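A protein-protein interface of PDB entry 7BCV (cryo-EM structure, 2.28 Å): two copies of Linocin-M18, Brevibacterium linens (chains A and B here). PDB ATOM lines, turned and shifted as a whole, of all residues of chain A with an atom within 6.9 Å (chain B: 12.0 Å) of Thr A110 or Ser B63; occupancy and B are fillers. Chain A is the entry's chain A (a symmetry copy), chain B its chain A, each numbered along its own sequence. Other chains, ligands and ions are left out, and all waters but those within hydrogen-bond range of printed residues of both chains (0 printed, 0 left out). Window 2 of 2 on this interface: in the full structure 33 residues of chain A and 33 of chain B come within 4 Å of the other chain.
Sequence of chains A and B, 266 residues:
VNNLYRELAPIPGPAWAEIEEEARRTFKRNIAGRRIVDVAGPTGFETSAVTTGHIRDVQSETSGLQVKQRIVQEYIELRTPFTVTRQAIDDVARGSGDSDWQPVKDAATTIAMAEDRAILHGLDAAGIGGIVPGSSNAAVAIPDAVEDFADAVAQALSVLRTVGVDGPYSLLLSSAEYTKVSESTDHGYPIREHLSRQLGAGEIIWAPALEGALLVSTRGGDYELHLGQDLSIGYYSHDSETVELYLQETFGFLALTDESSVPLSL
The backbone NH of Arg A79 lies within hydrogen-bond range of the backbone carbonyl oxygen of Gln B66 (2.8 Å).
Printed residues of chain A that touch a printed residue of chain B: Leu A78, Arg A79, Thr A80, Thr A110, Ala A114 and Arg A117.
Hydrophobic or aromatic side chains of chain A that line the printed part of chain B: Leu A78 and Ala A114.
Of chain B, only Ser B63 comes within 4 Å of Thr A110.
Thr A80 touches just these residues of chain B: Gly B64 (3.4 Å) and Leu B65 (3.9 Å).
No residue of chain B comes within 4 Å of Asp A106.
Printed residues of chain B within 4 Å of Ala A114: Leu B65 (3.7 Å).
Of the printed residues of chain B, Arg A79 touches Gly B64 (3.9 Å), Leu B65 (3.5 Å) and Gln B66 (2.8 Å).
Printed residues of chain A within 4 Å of Gly B64: Arg A79 and Thr A80.
Of the printed residues of chain A, Val B67 touches Leu A78 (3.9 Å).
Val A104 touches none of the printed residues of chain B.
Asn A30 touches none of the printed residues of chain B.
The nearest residue of chain A that does not touch Ser B63 is Thr A80 (6.2 Å).
The nearest printed residue of chain A that does not touch Thr B62 is Thr A110 (4.2 Å).
Gln B66 touches Leu A78.
Leu A78 touches Val B67.
O of Gly B64 touches O of Arg A79, 3.9 Å away.
Leu B65 touches Arg A79.
CG2 of Thr A80 touches O of Gly B64, 3.4 Å away.
Leu B65 touches Thr A80 (CD1 to CG2, 3.9 Å).
Ser B63 touches Thr A110 (O to CG2, 3.9 Å).
Leu B65 touches Ala A114 (CD2 to CB, 3.7 Å).
NH1 of Arg A117 touches OG1 of Thr B62, 3.8 Å away.
OG1 of Thr A80 is in hydrogen-bond range of O of Ala A107.
The backbone carbonyl oxygen (O) of Val B67 sits at hydrogen-bond distance from the backbone NH (N) of Val B58 (3.0 Å).
O of Asp A106 lies within hydrogen-bond range of OG1 of Thr A110 (2.9 Å).
The backbone NH (N) of Thr B62 is in hydrogen-bond range of the side-chain hydroxyl (OG) of Ser B60 (3.3 Å).
No position is printed for both chains.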
ATOM      1  N   THR A  26      18.208 -15.623 -23.479  1.00  0.00           N
ATOM      2  CA  THR A  26      17.136 -15.416 -24.441  1.00  0.00           C
ATOM      3  C   THR A  26      15.820 -16.003 -23.947  1.00  0.00           C
ATOM      4  O   THR A  26      14.765 -15.384 -24.118  1.00  0.00           O
ATOM      5  CB  THR A  26      17.547 -16.009 -25.790  1.00  0.00           C
ATOM      6  OG1 THR A  26      18.701 -15.317 -26.277  1.00  0.00           O
ATOM      7  CG2 THR A  26      16.442 -15.908 -26.812  1.00  0.00           C
ATOM      8  N   ASN A  30      11.953 -13.944 -22.848  1.00  0.00           N
ATOM      9  CA  ASN A  30      10.795 -14.232 -23.674  1.00  0.00           C
ATOM     10  C   ASN A  30       9.718 -15.032 -22.960  1.00  0.00           C
ATOM     11  O   ASN A  30       8.662 -15.256 -23.550  1.00  0.00           O
ATOM     12  CB  ASN A  30      11.213 -14.988 -24.943  1.00  0.00           C
ATOM     13  CG  ASN A  30      11.687 -14.068 -26.045  1.00  0.00           C
ATOM     14  OD1 ASN A  30      10.888 -13.435 -26.725  1.00  0.00           O
ATOM     15  ND2 ASN A  30      12.991 -14.007 -26.244  1.00  0.00           N
ATOM     16  N   LEU A  78       8.591 -30.485 -24.783  1.00  0.00           N
ATOM     17  CA  LEU A  78       8.856 -29.566 -25.878  1.00  0.00           C
ATOM     18  C   LEU A  78      10.315 -29.718 -26.286  1.00  0.00           C
ATOM     19  O   LEU A  78      11.192 -29.737 -25.427  1.00  0.00           O
ATOM     20  CB  LEU A  78       8.572 -28.119 -25.465  1.00  0.00           C
ATOM     21  CG  LEU A  78       7.157 -27.688 -25.076  1.00  0.00           C
ATOM     22  CD1 LEU A  78       7.102 -26.197 -24.787  1.00  0.00           C
ATOM     23  CD2 LEU A  78       6.163 -28.057 -26.160  1.00  0.00           C
ATOM     24  N   ARG A  79      10.572 -29.831 -27.584  1.00  0.00           N
ATOM     25  CA  ARG A  79      11.943 -29.914 -28.070  1.00  0.00           C
ATOM     26  C   ARG A  79      12.159 -28.990 -29.259  1.00  0.00           C
ATOM     27  O   ARG A  79      11.435 -29.075 -30.252  1.00  0.00           O
ATOM     28  CB  ARG A  79      12.319 -31.348 -28.452  1.00  0.00           C
ATOM     29  CG  ARG A  79      13.813 -31.545 -28.594  1.00  0.00           C
ATOM     30  CD  ARG A  79      14.168 -32.924 -29.062  1.00  0.00           C
ATOM     31  NE  ARG A  79      14.367 -33.821 -27.942  1.00  0.00           N
ATOM     32  CZ  ARG A  79      14.972 -34.993 -28.020  1.00  0.00           C
ATOM     33  NH1 ARG A  79      15.103 -35.740 -26.936  1.00  0.00           N
ATOM     34  NH2 ARG A  79      15.447 -35.406 -29.182  1.00  0.00           N
ATOM     35  N   THR A  80      13.155 -28.117 -29.158  1.00  0.00           N
ATOM     36  CA  THR A  80      13.563 -27.266 -30.275  1.00  0.00           C
ATOM     37  C   THR A  80      14.992 -27.576 -30.680  1.00  0.00           C
ATOM     38  O   THR A  80      15.931 -27.197 -29.957  1.00  0.00           O
ATOM     39  CB  THR A  80      13.429 -25.783 -29.934  1.00  0.00           C
ATOM     40  OG1 THR A  80      14.125 -25.492 -28.716  1.00  0.00           O
ATOM     41  CG2 THR A  80      11.973 -25.401 -29.807  1.00  0.00           C
ATOM     42  N   VAL A 104      21.058 -20.735 -31.408  1.00  0.00           N
ATOM     43  CA  VAL A 104      20.585 -21.142 -30.092  1.00  0.00           C
ATOM     44  C   VAL A 104      19.602 -20.091 -29.599  1.00  0.00           C
ATOM     45  O   VAL A 104      18.631 -20.416 -28.915  1.00  0.00           O
ATOM     46  CB  VAL A 104      21.746 -21.361 -29.093  1.00  0.00           C
ATOM     47  CG1 VAL A 104      23.093 -21.487 -29.799  1.00  0.00           C
ATOM     48  CG2 VAL A 104      21.730 -20.453 -27.852  1.00  0.00           C
ATOM     49  N   LYS A 105      19.805 -18.839 -30.018  1.00  0.00           N
ATOM     50  CA  LYS A 105      18.908 -17.752 -29.663  1.00  0.00           C
ATOM     51  C   LYS A 105      17.554 -17.923 -30.334  1.00  0.00           C
ATOM     52  O   LYS A 105      16.513 -17.704 -29.703  1.00  0.00           O
ATOM     53  CB  LYS A 105      19.550 -16.423 -30.048  1.00  0.00           C
ATOM     54  CG  LYS A 105      18.707 -15.210 -29.795  1.00  0.00           C
ATOM     55  CD  LYS A 105      19.499 -13.951 -30.066  1.00  0.00           C
ATOM     56  CE  LYS A 105      18.717 -12.720 -29.684  1.00  0.00           C
ATOM     57  NZ  LYS A 105      19.613 -11.564 -29.437  1.00  0.00           N
ATOM     58  N   ASP A 106      17.557 -18.361 -31.597  1.00  0.00           N
ATOM     59  CA  ASP A 106      16.312 -18.638 -32.303  1.00  0.00           C
ATOM     60  C   ASP A 106      15.576 -19.816 -31.679  1.00  0.00           C
ATOM     61  O   ASP A 106      14.352 -19.770 -31.515  1.00  0.00           O
ATOM     62  CB  ASP A 106      16.585 -18.896 -33.779  1.00  0.00           C
ATOM     63  CG  ASP A 106      17.158 -17.688 -34.484  1.00  0.00           C
ATOM     64  OD1 ASP A 106      17.102 -16.582 -33.910  1.00  0.00           O
ATOM     65  OD2 ASP A 106      17.679 -17.838 -35.606  1.00  0.00           O
ATOM     66  N   ALA A 107      16.318 -20.851 -31.274  1.00  0.00           N
ATOM     67  CA  ALA A 107      15.719 -21.997 -30.601  1.00  0.00           C
ATOM     68  C   ALA A 107      15.155 -21.625 -29.230  1.00  0.00           C
ATOM     69  O   ALA A 107      14.088 -22.117 -28.848  1.00  0.00           O
ATOM     70  CB  ALA A 107      16.750 -23.117 -30.478  1.00  0.00           C
ATOM     71  N   ALA A 108      15.847 -20.763 -28.480  1.00  0.00           N
ATOM     72  CA  ALA A 108      15.361 -20.360 -27.166  1.00  0.00           C
ATOM     73  C   ALA A 108      14.116 -19.497 -27.283  1.00  0.00           C
ATOM     74  O   ALA A 108      13.187 -19.640 -26.483  1.00  0.00           O
ATOM     75  CB  ALA A 108      16.455 -19.633 -26.387  1.00  0.00           C
ATOM     76  N   THR A 109      14.070 -18.644 -28.311  1.00  0.00           N
ATOM     77  CA  THR A 109      12.877 -17.862 -28.603  1.00  0.00           C
ATOM     78  C   THR A 109      11.699 -18.759 -28.961  1.00  0.00           C
ATOM     79  O   THR A 109      10.592 -18.563 -28.449  1.00  0.00           O
ATOM     80  CB  THR A 109      13.188 -16.874 -29.730  1.00  0.00           C
ATOM     81  OG1 THR A 109      14.141 -15.916 -29.267  1.00  0.00           O
ATOM     82  CG2 THR A 109      11.953 -16.153 -30.201  1.00  0.00           C
ATOM     83  N   THR A 110      11.943 -19.788 -29.783  1.00  0.00           N
ATOM     84  CA  THR A 110      10.887 -20.714 -30.190  1.00  0.00           C
ATOM     85  C   THR A 110      10.347 -21.525 -29.010  1.00  0.00           C
ATOM     86  O   THR A 110       9.128 -21.652 -28.854  1.00  0.00           O
ATOM     87  CB  THR A 110      11.413 -21.634 -31.294  1.00  0.00           C
ATOM     88  OG1 THR A 110      11.848 -20.845 -32.404  1.00  0.00           O
ATOM     89  CG2 THR A 110      10.356 -22.606 -31.767  1.00  0.00           C
ATOM     90  N   ILE A 111      11.224 -22.030 -28.142  1.00  0.00           N
ATOM     91  CA  ILE A 111      10.739 -22.857 -27.041  1.00  0.00           C
ATOM     92  C   ILE A 111      10.067 -22.001 -25.957  1.00  0.00           C
ATOM     93  O   ILE A 111       9.065 -22.429 -25.370  1.00  0.00           O
ATOM     94  CB  ILE A 111      11.867 -23.773 -26.497  1.00  0.00           C
ATOM     95  CG1 ILE A 111      11.276 -25.011 -25.823  1.00  0.00           C
ATOM     96  CG2 ILE A 111      12.800 -23.088 -25.538  1.00  0.00           C
ATOM     97  CD1 ILE A 111      12.300 -26.094 -25.477  1.00  0.00           C
ATOM     98  N   ALA A 112      10.530 -20.759 -25.741  1.00  0.00           N
ATOM     99  CA  ALA A 112       9.871 -19.862 -24.799  1.00  0.00           C
ATOM    100  C   ALA A 112       8.491 -19.452 -25.296  1.00  0.00           C
ATOM    101  O   ALA A 112       7.532 -19.392 -24.513  1.00  0.00           O
ATOM    102  CB  ALA A 112      10.745 -18.635 -24.562  1.00  0.00           C
ATOM    103  N   MET A 113       8.365 -19.229 -26.603  1.00  0.00           N
ATOM    104  CA  MET A 113       7.073 -18.880 -27.170  1.00  0.00           C
ATOM    105  C   MET A 113       6.126 -20.070 -27.179  1.00  0.00           C
ATOM    106  O   MET A 113       4.928 -19.889 -26.974  1.00  0.00           O
ATOM    107  CB  MET A 113       7.261 -18.310 -28.574  1.00  0.00           C
ATOM    108  CG  MET A 113       7.766 -16.868 -28.558  1.00  0.00           C
ATOM    109  SD  MET A 113       7.642 -15.980 -30.115  1.00  0.00           S
ATOM    110  CE  MET A 113       5.878 -15.771 -30.245  1.00  0.00           C
ATOM    111  N   ALA A 114       6.644 -21.286 -27.356  1.00  0.00           N
ATOM    112  CA  ALA A 114       5.804 -22.475 -27.268  1.00  0.00           C
ATOM    113  C   ALA A 114       5.313 -22.708 -25.846  1.00  0.00           C
ATOM    114  O   ALA A 114       4.159 -23.103 -25.642  1.00  0.00           O
ATOM    115  CB  ALA A 114       6.564 -23.696 -27.774  1.00  0.00           C
ATOM    116  N   GLU A 115       6.165 -22.449 -24.854  1.00  0.00           N
ATOM    117  CA  GLU A 115       5.758 -22.637 -23.467  1.00  0.00           C
ATOM    118  C   GLU A 115       4.687 -21.629 -23.063  1.00  0.00           C
ATOM    119  O   GLU A 115       3.673 -22.003 -22.455  1.00  0.00           O
ATOM    120  CB  GLU A 115       6.966 -22.536 -22.541  1.00  0.00           C
ATOM    121  CG  GLU A 115       6.665 -22.953 -21.112  1.00  0.00           C
ATOM    122  CD  GLU A 115       7.519 -22.228 -20.092  1.00  0.00           C
ATOM    123  OE1 GLU A 115       8.012 -21.135 -20.405  1.00  0.00           O
ATOM    124  OE2 GLU A 115       7.714 -22.757 -18.982  1.00  0.00           O
ATOM    125  N   ARG A 117       2.707 -20.112 -25.173  1.00  0.00           N
ATOM    126  CA  ARG A 117       1.517 -20.407 -25.954  1.00  0.00           C
ATOM    127  C   ARG A 117       0.727 -21.558 -25.352  1.00  0.00           C
ATOM    128  O   ARG A 117      -0.502 -21.567 -25.437  1.00  0.00           O
ATOM    129  CB  ARG A 117       1.914 -20.716 -27.391  1.00  0.00           C
ATOM    130  CG  ARG A 117       0.805 -20.601 -28.407  1.00  0.00           C
ATOM    131  CD  ARG A 117       1.400 -20.491 -29.791  1.00  0.00           C
ATOM    132  NE  ARG A 117       2.646 -19.729 -29.741  1.00  0.00           N
ATOM    133  CZ  ARG A 117       3.523 -19.638 -30.732  1.00  0.00           C
ATOM    134  NH1 ARG A 117       3.312 -20.259 -31.883  1.00  0.00           N
ATOM    135  NH2 ARG A 117       4.621 -18.918 -30.567  1.00  0.00           N
ATOM    136  N   VAL B  58       2.557 -35.355 -30.407  1.00  0.00           N
ATOM    137  CA  VAL B  58       1.495 -34.361 -30.354  1.00  0.00           C
ATOM    138  C   VAL B  58       1.584 -33.518 -31.613  1.00  0.00           C
ATOM    139  O   VAL B  58       2.682 -33.167 -32.059  1.00  0.00           O
ATOM    140  CB  VAL B  58       1.613 -33.496 -29.084  1.00  0.00           C
ATOM    141  CG1 VAL B  58       0.419 -32.579 -28.916  1.00  0.00           C
ATOM    142  CG2 VAL B  58       1.773 -34.376 -27.875  1.00  0.00           C
ATOM    143  N   GLN B  59       0.434 -33.204 -32.197  1.00  0.00           N
ATOM    144  CA  GLN B  59       0.393 -32.411 -33.416  1.00  0.00           C
ATOM    145  C   GLN B  59       0.775 -30.963 -33.128  1.00  0.00           C
ATOM    146  O   GLN B  59       0.189 -30.317 -32.255  1.00  0.00           O
ATOM    147  CB  GLN B  59      -0.998 -32.487 -34.042  1.00  0.00           C
ATOM    148  CG  GLN B  59      -1.271 -31.570 -35.246  1.00  0.00           C
ATOM    149  CD  GLN B  59      -0.574 -31.981 -36.546  1.00  0.00           C
ATOM    150  OE1 GLN B  59       0.646 -32.138 -36.609  1.00  0.00           O
ATOM    151  NE2 GLN B  59      -1.365 -32.159 -37.596  1.00  0.00           N
ATOM    152  N   SER B  60       1.762 -30.461 -33.860  1.00  0.00           N
ATOM    153  CA  SER B  60       2.204 -29.082 -33.744  1.00  0.00           C
ATOM    154  C   SER B  60       2.512 -28.544 -35.133  1.00  0.00           C
ATOM    155  O   SER B  60       2.979 -29.286 -36.001  1.00  0.00           O
ATOM    156  CB  SER B  60       3.438 -28.971 -32.841  1.00  0.00           C
ATOM    157  OG  SER B  60       4.100 -27.736 -33.025  1.00  0.00           O
ATOM    158  N   GLU B  61       2.246 -27.260 -35.344  1.00  0.00           N
ATOM    159  CA  GLU B  61       2.542 -26.619 -36.617  1.00  0.00           C
ATOM    160  C   GLU B  61       3.627 -25.554 -36.517  1.00  0.00           C
ATOM    161  O   GLU B  61       3.963 -24.938 -37.531  1.00  0.00           O
ATOM    162  CB  GLU B  61       1.270 -26.006 -37.214  1.00  0.00           C
ATOM    163  CG  GLU B  61       0.194 -27.008 -37.631  1.00  0.00           C
ATOM    164  CD  GLU B  61       0.643 -28.030 -38.677  1.00  0.00           C
ATOM    165  OE1 GLU B  61       0.043 -29.125 -38.712  1.00  0.00           O
ATOM    166  OE2 GLU B  61       1.548 -27.742 -39.490  1.00  0.00           O
ATOM    167  N   THR B  62       4.186 -25.334 -35.331  1.00  0.00           N
ATOM    168  CA  THR B  62       5.299 -24.406 -35.177  1.00  0.00           C
ATOM    169  C   THR B  62       6.557 -24.988 -35.810  1.00  0.00           C
ATOM    170  O   THR B  62       6.886 -26.160 -35.599  1.00  0.00           O
ATOM    171  CB  THR B  62       5.536 -24.114 -33.695  1.00  0.00           C
ATOM    172  OG1 THR B  62       4.317 -23.665 -33.093  1.00  0.00           O
ATOM    173  CG2 THR B  62       6.603 -23.050 -33.493  1.00  0.00           C
ATOM    174  N   SER B  63       7.250 -24.171 -36.600  1.00  0.00           N
ATOM    175  CA  SER B  63       8.469 -24.608 -37.267  1.00  0.00           C
ATOM    176  C   SER B  63       9.585 -24.819 -36.253  1.00  0.00           C
ATOM    177  O   SER B  63       9.855 -23.952 -35.420  1.00  0.00           O
ATOM    178  CB  SER B  63       8.892 -23.582 -38.317  1.00  0.00           C
ATOM    179  OG  SER B  63      10.090 -23.972 -38.961  1.00  0.00           O
ATOM    180  N   GLY B  64      10.220 -25.985 -36.315  1.00  0.00           N
ATOM    181  CA  GLY B  64      11.315 -26.282 -35.417  1.00  0.00           C
ATOM    182  C   GLY B  64      10.915 -26.605 -33.998  1.00  0.00           C
ATOM    183  O   GLY B  64      11.701 -26.371 -33.077  1.00  0.00           O
ATOM    184  N   LEU B  65       9.714 -27.139 -33.790  1.00  0.00           N
ATOM    185  CA  LEU B  65       9.222 -27.488 -32.466  1.00  0.00           C
ATOM    186  C   LEU B  65       8.612 -28.880 -32.500  1.00  0.00           C
ATOM    187  O   LEU B  65       7.714 -29.149 -33.302  1.00  0.00           O
ATOM    188  CB  LEU B  65       8.193 -26.469 -31.970  1.00  0.00           C
ATOM    189  CG  LEU B  65       7.425 -26.856 -30.706  1.00  0.00           C
ATOM    190  CD1 LEU B  65       8.279 -26.683 -29.461  1.00  0.00           C
ATOM    191  CD2 LEU B  65       6.140 -26.063 -30.603  1.00  0.00           C
ATOM    192  N   GLN B  66       9.096 -29.758 -31.634  1.00  0.00           N
ATOM    193  CA  GLN B  66       8.573 -31.108 -31.505  1.00  0.00           C
ATOM    194  C   GLN B  66       7.901 -31.240 -30.148  1.00  0.00           C
ATOM    195  O   GLN B  66       8.493 -30.890 -29.124  1.00  0.00           O
ATOM    196  CB  GLN B  66       9.684 -32.151 -31.664  1.00  0.00           C
ATOM    197  CG  GLN B  66      10.320 -32.185 -33.047  1.00  0.00           C
ATOM    198  CD  GLN B  66      11.780 -32.602 -33.008  1.00  0.00           C
ATOM    199  OE1 GLN B  66      12.294 -32.997 -31.969  1.00  0.00           O
ATOM    200  NE2 GLN B  66      12.448 -32.521 -34.143  1.00  0.00           N
ATOM    201  N   VAL B  67       6.665 -31.725 -30.138  1.00  0.00           N
ATOM    202  CA  VAL B  67       5.905 -31.900 -28.907  1.00  0.00           C
ATOM    203  C   VAL B  67       5.622 -33.379 -28.710  1.00  0.00           C
ATOM    204  O   VAL B  67       5.078 -34.039 -29.600  1.00  0.00           O
ATOM    205  CB  VAL B  67       4.595 -31.093 -28.909  1.00  0.00           C
ATOM    206  CG1 VAL B  67       4.012 -31.063 -27.510  1.00  0.00           C
ATOM    207  CG2 VAL B  67       4.831 -29.692 -29.401  1.00  0.00           C
